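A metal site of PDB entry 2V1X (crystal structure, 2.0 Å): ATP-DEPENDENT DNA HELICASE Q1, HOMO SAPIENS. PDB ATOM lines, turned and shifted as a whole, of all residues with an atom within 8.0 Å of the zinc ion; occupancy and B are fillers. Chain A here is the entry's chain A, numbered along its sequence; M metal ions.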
ATOM      1  N   LEU A 239      -6.595  -2.264  23.657  1.00  0.00           N
ATOM      2  CA  LEU A 239      -7.699  -1.604  22.972  1.00  0.00           C
ATOM      3  C   LEU A 239      -7.510  -0.104  23.005  1.00  0.00           C
ATOM      4  O   LEU A 239      -7.239   0.502  24.065  1.00  0.00           O
ATOM      5  CB  LEU A 239      -9.035  -2.002  23.611  1.00  0.00           C
ATOM      6  CG  LEU A 239      -9.465  -3.454  23.408  1.00  0.00           C
ATOM      7  CD1 LEU A 239     -10.889  -3.651  23.897  1.00  0.00           C
ATOM      8  CD2 LEU A 239      -9.319  -3.892  21.938  1.00  0.00           C
ATOM      9  N   TYR A 240      -7.565   0.523  21.839  1.00  0.00           N
ATOM     10  CA  TYR A 240      -7.526   1.984  21.805  1.00  0.00           C
ATOM     11  C   TYR A 240      -8.973   2.478  21.814  1.00  0.00           C
ATOM     12  O   TYR A 240      -9.756   2.134  20.920  1.00  0.00           O
ATOM     13  CB  TYR A 240      -6.771   2.520  20.595  1.00  0.00           C
ATOM     14  CG  TYR A 240      -6.581   4.031  20.672  1.00  0.00           C
ATOM     15  CD1 TYR A 240      -5.546   4.565  21.418  1.00  0.00           C
ATOM     16  CD2 TYR A 240      -7.461   4.907  20.036  1.00  0.00           C
ATOM     17  CE1 TYR A 240      -5.372   5.926  21.521  1.00  0.00           C
ATOM     18  CE2 TYR A 240      -7.277   6.283  20.126  1.00  0.00           C
ATOM     19  CZ  TYR A 240      -6.242   6.781  20.867  1.00  0.00           C
ATOM     20  OH  TYR A 240      -6.058   8.137  20.979  1.00  0.00           O
ATOM     21  N   TYR A 241      -9.300   3.278  22.822  1.00  0.00           N
ATOM     22  CA  TYR A 241     -10.666   3.833  22.981  1.00  0.00           C
ATOM     23  C   TYR A 241     -10.732   5.319  22.603  1.00  0.00           C
ATOM     24  O   TYR A 241     -10.051   6.184  23.195  1.00  0.00           O
ATOM     25  CB  TYR A 241     -11.189   3.651  24.397  1.00  0.00           C
ATOM     26  CG  TYR A 241     -11.467   2.222  24.834  1.00  0.00           C
ATOM     27  CD1 TYR A 241     -12.443   1.450  24.210  1.00  0.00           C
ATOM     28  CD2 TYR A 241     -10.777   1.655  25.888  1.00  0.00           C
ATOM     29  CE1 TYR A 241     -12.705   0.151  24.645  1.00  0.00           C
ATOM     30  CE2 TYR A 241     -11.039   0.356  26.322  1.00  0.00           C
ATOM     31  CZ  TYR A 241     -11.981  -0.397  25.685  1.00  0.00           C
ATOM     32  OH  TYR A 241     -12.243  -1.708  26.113  1.00  0.00           O
ATOM     33  N   SER A 404     -11.603  15.248  29.215  1.00  0.00           N
ATOM     34  CA  SER A 404     -10.416  15.136  30.049  1.00  0.00           C
ATOM     35  C   SER A 404     -10.138  13.712  30.575  1.00  0.00           C
ATOM     36  O   SER A 404      -9.015  13.221  30.436  1.00  0.00           O
ATOM     37  CB  SER A 404     -10.532  16.097  31.215  1.00  0.00           C
ATOM     38  OG  SER A 404     -11.552  15.668  32.101  1.00  0.00           O
ATOM     39  N   LYS A 405     -11.132  13.066  31.171  1.00  0.00           N
ATOM     40  CA  LYS A 405     -10.938  11.812  31.893  1.00  0.00           C
ATOM     41  C   LYS A 405     -10.567  10.619  31.011  1.00  0.00           C
ATOM     42  O   LYS A 405     -11.083  10.452  29.908  1.00  0.00           O
ATOM     43  CB  LYS A 405     -12.195  11.432  32.706  1.00  0.00           C
ATOM     44  CG  LYS A 405     -12.382  12.233  34.016  1.00  0.00           C
ATOM     45  CD  LYS A 405     -11.659  11.622  35.212  1.00  0.00           C
ATOM     46  CE  LYS A 405     -11.564  12.628  36.352  1.00  0.00           C
ATOM     47  N   CYS A 406      -9.666   9.796  31.548  1.00  0.00           N
ATOM     48  CA  CYS A 406      -9.255   8.559  30.891  1.00  0.00           C
ATOM     49  C   CYS A 406     -10.460   7.677  30.608  1.00  0.00           C
ATOM     50  O   CYS A 406     -11.302   7.504  31.470  1.00  0.00           O
ATOM     51  CB  CYS A 406      -8.258   7.817  31.794  1.00  0.00           C
ATOM     52  SG  CYS A 406      -7.680   6.235  31.118  1.00  0.00           S
ATOM     53  N   ARG A 407     -10.541   7.117  29.420  1.00  0.00           N
ATOM     54  CA  ARG A 407     -11.693   6.319  29.030  1.00  0.00           C
ATOM     55  C   ARG A 407     -11.894   5.094  29.887  1.00  0.00           C
ATOM     56  O   ARG A 407     -13.033   4.713  30.190  1.00  0.00           O
ATOM     57  CB  ARG A 407     -11.548   5.880  27.559  1.00  0.00           C
ATOM     58  CG  ARG A 407     -11.507   7.035  26.582  1.00  0.00           C
ATOM     59  CD  ARG A 407     -12.834   7.701  26.467  1.00  0.00           C
ATOM     60  NE  ARG A 407     -12.874   8.780  25.494  1.00  0.00           N
ATOM     61  CZ  ARG A 407     -13.739   9.796  25.551  1.00  0.00           C
ATOM     62  NH1 ARG A 407     -14.662   9.846  26.504  1.00  0.00           N
ATOM     63  NH2 ARG A 407     -13.711  10.767  24.653  1.00  0.00           N
ATOM     64  N   ARG A 408     -10.769   4.473  30.246  1.00  0.00           N
ATOM     65  CA  ARG A 408     -10.698   3.324  31.143  1.00  0.00           C
ATOM     66  C   ARG A 408     -11.118   3.665  32.538  1.00  0.00           C
ATOM     67  O   ARG A 408     -11.772   2.877  33.195  1.00  0.00           O
ATOM     68  CB  ARG A 408      -9.270   2.762  31.155  1.00  0.00           C
ATOM     69  CG  ARG A 408      -8.932   1.988  29.906  1.00  0.00           C
ATOM     70  CD  ARG A 408      -7.493   1.462  29.832  1.00  0.00           C
ATOM     71  NE  ARG A 408      -7.432   0.365  28.863  1.00  0.00           N
ATOM     72  CZ  ARG A 408      -7.395   0.520  27.546  1.00  0.00           C
ATOM     73  NH1 ARG A 408      -7.370  -0.556  26.779  1.00  0.00           N
ATOM     74  NH2 ARG A 408      -7.360   1.730  26.997  1.00  0.00           N
ATOM     75  N   VAL A 409     -10.739   4.851  33.004  1.00  0.00           N
ATOM     76  CA  VAL A 409     -11.166   5.360  34.301  1.00  0.00           C
ATOM     77  C   VAL A 409     -12.697   5.512  34.385  1.00  0.00           C
ATOM     78  O   VAL A 409     -13.300   5.217  35.419  1.00  0.00           O
ATOM     79  CB  VAL A 409     -10.478   6.711  34.607  1.00  0.00           C
ATOM     80  CG1 VAL A 409     -11.194   7.490  35.726  1.00  0.00           C
ATOM     81  CG2 VAL A 409      -9.010   6.469  34.958  1.00  0.00           C
ATOM     82  N   LEU A 410     -13.295   5.931  33.267  1.00  0.00           N
ATOM     83  CA  LEU A 410     -14.746   6.155  33.164  1.00  0.00           C
ATOM     84  C   LEU A 410     -15.468   4.835  33.104  1.00  0.00           C
ATOM     85  O   LEU A 410     -16.491   4.679  33.748  1.00  0.00           O
ATOM     86  CB  LEU A 410     -15.095   6.999  31.923  1.00  0.00           C
ATOM     87  CG  LEU A 410     -14.603   8.449  31.937  1.00  0.00           C
ATOM     88  CD1 LEU A 410     -14.873   9.176  30.598  1.00  0.00           C
ATOM     89  CD2 LEU A 410     -15.188   9.226  33.105  1.00  0.00           C
ATOM     90  N   TRP A 419      -9.173  -0.681  39.930  1.00  0.00           N
ATOM     91  CA  TRP A 419      -8.363  -0.012  38.882  1.00  0.00           C
ATOM     92  C   TRP A 419      -7.018   0.541  39.409  1.00  0.00           C
ATOM     93  O   TRP A 419      -6.869   1.737  39.660  1.00  0.00           O
ATOM     94  CB  TRP A 419      -9.198   1.085  38.180  1.00  0.00           C
ATOM     95  CG  TRP A 419      -8.564   1.656  36.936  1.00  0.00           C
ATOM     96  CD1 TRP A 419      -8.304   2.966  36.668  1.00  0.00           C
ATOM     97  CD2 TRP A 419      -8.102   0.916  35.806  1.00  0.00           C
ATOM     98  NE1 TRP A 419      -7.712   3.101  35.442  1.00  0.00           N
ATOM     99  CE2 TRP A 419      -7.579   1.852  34.888  1.00  0.00           C
ATOM    100  CE3 TRP A 419      -8.076  -0.439  35.471  1.00  0.00           C
ATOM    101  CZ2 TRP A 419      -7.035   1.469  33.652  1.00  0.00           C
ATOM    102  CZ3 TRP A 419      -7.540  -0.821  34.262  1.00  0.00           C
ATOM    103  CH2 TRP A 419      -7.022   0.128  33.364  1.00  0.00           C
ATOM    104  N   ALA A 423      -3.423   1.966  34.997  1.00  0.00           N
ATOM    105  CA  ALA A 423      -2.388   2.033  33.965  1.00  0.00           C
ATOM    106  C   ALA A 423      -2.958   1.919  32.552  1.00  0.00           C
ATOM    107  O   ALA A 423      -3.088   0.816  32.009  1.00  0.00           O
ATOM    108  CB  ALA A 423      -1.357   0.922  34.199  1.00  0.00           C
ATOM    109  N   CYS A 424      -3.291   3.064  31.967  1.00  0.00           N
ATOM    110  CA  CYS A 424      -3.787   3.112  30.580  1.00  0.00           C
ATOM    111  C   CYS A 424      -2.639   3.092  29.590  1.00  0.00           C
ATOM    112  O   CYS A 424      -2.725   2.460  28.529  1.00  0.00           O
ATOM    113  CB  CYS A 424      -4.573   4.396  30.358  1.00  0.00           C
ATOM    114  SG  CYS A 424      -5.385   4.542  28.751  1.00  0.00           S
ATOM    115  N   ASN A 425      -1.594   3.846  29.932  1.00  0.00           N
ATOM    116  CA  ASN A 425      -0.389   3.969  29.096  1.00  0.00           C
ATOM    117  C   ASN A 425      -0.693   4.531  27.713  1.00  0.00           C
ATOM    118  O   ASN A 425      -0.394   3.903  26.688  1.00  0.00           O
ATOM    119  CB  ASN A 425       0.343   2.616  28.999  1.00  0.00           C
ATOM    120  CG  ASN A 425       0.719   2.058  30.358  1.00  0.00           C
ATOM    121  OD1 ASN A 425       1.059   2.812  31.282  1.00  0.00           O
ATOM    122  ND2 ASN A 425       0.653   0.738  30.501  1.00  0.00           N
ATOM    123  N   LYS A 426      -1.314   5.701  27.694  1.00  0.00           N
ATOM    124  CA  LYS A 426      -1.705   6.369  26.443  1.00  0.00           C
ATOM    125  C   LYS A 426      -2.478   5.473  25.433  1.00  0.00           C
ATOM    126  O   LYS A 426      -2.158   5.437  24.231  1.00  0.00           O
ATOM    127  CB  LYS A 426      -0.467   6.989  25.782  1.00  0.00           C
ATOM    128  CG  LYS A 426       0.480   7.719  26.737  1.00  0.00           C
ATOM    129  CD  LYS A 426      -0.208   8.838  27.502  1.00  0.00           C
ATOM    130  CE  LYS A 426       0.798   9.709  28.267  1.00  0.00           C
ATOM    131  NZ  LYS A 426       1.498   8.964  29.362  1.00  0.00           N
ATOM    132  N   MET A 427      -3.508   4.773  25.890  1.00  0.00           N
ATOM    133  CA  MET A 427      -4.309   3.911  25.010  1.00  0.00           C
ATOM    134  C   MET A 427      -5.798   4.363  24.951  1.00  0.00           C
ATOM    135  O   MET A 427      -6.709   3.568  24.800  1.00  0.00           O
ATOM    136  CB  MET A 427      -4.171   2.458  25.434  1.00  0.00           C
ATOM    137  CG  MET A 427      -2.811   1.821  25.088  1.00  0.00           C
ATOM    138  SD  MET A 427      -2.602   1.577  23.324  1.00  0.00           S
ATOM    139  CE  MET A 427      -3.658   0.212  22.834  1.00  0.00           C
ATOM    140  N   CYS A 428      -6.017   5.673  25.047  1.00  0.00           N
ATOM    141  CA  CYS A 428      -7.306   6.258  24.785  1.00  0.00           C
ATOM    142  C   CYS A 428      -7.079   7.692  24.356  1.00  0.00           C
ATOM    143  O   CYS A 428      -6.050   8.287  24.680  1.00  0.00           O
ATOM    144  CB  CYS A 428      -8.196   6.188  26.032  1.00  0.00           C
ATOM    145  SG  CYS A 428      -7.879   7.385  27.272  1.00  0.00           S
ATOM    146  N   ASP A 429      -8.046   8.248  23.625  1.00  0.00           N
ATOM    147  CA  ASP A 429      -7.894   9.604  23.114  1.00  0.00           C
ATOM    148  C   ASP A 429      -7.605  10.647  24.179  1.00  0.00           C
ATOM    149  O   ASP A 429      -6.814  11.530  23.934  1.00  0.00           O
ATOM    150  CB  ASP A 429      -9.086  10.026  22.278  1.00  0.00           C
ATOM    151  CG  ASP A 429     -10.404   9.877  22.997  1.00  0.00           C
ATOM    152  OD1 ASP A 429     -11.420  10.151  22.340  1.00  0.00           O
ATOM    153  OD2 ASP A 429     -10.426   9.458  24.177  1.00  0.00           O
ATOM    154  N   ASN A 430      -8.206  10.529  25.351  1.00  0.00           N
ATOM    155  CA  ASN A 430      -8.012  11.566  26.391  1.00  0.00           C
ATOM    156  C   ASN A 430      -6.691  11.500  27.148  1.00  0.00           C
ATOM    157  O   ASN A 430      -6.244  12.502  27.729  1.00  0.00           O
ATOM    158  CB  ASN A 430      -9.166  11.551  27.403  1.00  0.00           C
ATOM    159  CG  ASN A 430     -10.498  12.008  26.799  1.00  0.00           C
ATOM    160  OD1 ASN A 430     -10.539  12.588  25.712  1.00  0.00           O
ATOM    161  ND2 ASN A 430     -11.591  11.720  27.498  1.00  0.00           N
ATOM    162  N   CYS A 431      -6.057  10.326  27.162  1.00  0.00           N
ATOM    163  CA  CYS A 431      -4.768  10.172  27.835  1.00  0.00           C
ATOM    164  C   CYS A 431      -3.632  10.722  26.989  1.00  0.00           C
ATOM    165  O   CYS A 431      -2.603  11.145  27.526  1.00  0.00           O
ATOM    166  CB  CYS A 431      -4.508   8.713  28.204  1.00  0.00           C
ATOM    167  SG  CYS A 431      -5.335   8.220  29.708  1.00  0.00           S
ATOM    168  N   CYS A 432      -3.852  10.713  25.685  1.00  0.00           N
ATOM    169  CA  CYS A 432      -2.893  11.230  24.720  1.00  0.00           C
ATOM    170  C   CYS A 432      -2.941  12.756  24.521  1.00  0.00           C
ATOM    171  O   CYS A 432      -1.997  13.337  23.996  1.00  0.00           O
ATOM    172  CB  CYS A 432      -3.109  10.525  23.380  1.00  0.00           C
ATOM    173  SG  CYS A 432      -2.853   8.753  23.499  1.00  0.00           S
HETATM  174 ZN    ZN M   1      -6.692   6.482  29.017  1.00  0.00          ZN
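The zinc ion is bound by SG of Cys 428, SG of Cys 431, SG of Cys 406 and SG of Cys 424. The zinc ion has four donor atoms within binding distance.
Merely in contact with the zinc ion: Arg 407 (3.9 Å). Five residues have an atom within 4 Å of the zinc ion: Cys 406, Arg 407, Cys 424, Cys 428 and Cys 431.
O of Cys 428 is in hydrogen-bond range of SG of Cys 432 (3.4 Å). The backbone NH of Arg 407 lies close to the side-chain sulfur of Cys 428, 3.4 Å away. The side-chain sulfur (SG) of Cys 406 sits close to the backbone NH (N) of Arg 408, at 3.7 Å. The side-chain sulfur (SG) of Cys 428 sits close to the backbone NH (N) of Asn 430 (3.7 Å). The backbone NH (N) of Met 427 lies close to the side-chain sulfur (SG) of Cys 424, 3.4 Å away. The guanidinium group (NE) of Arg 407 lies within salt-bridge range of the side-chain carboxylate (OD2) of Asp 429 (2.9 Å).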
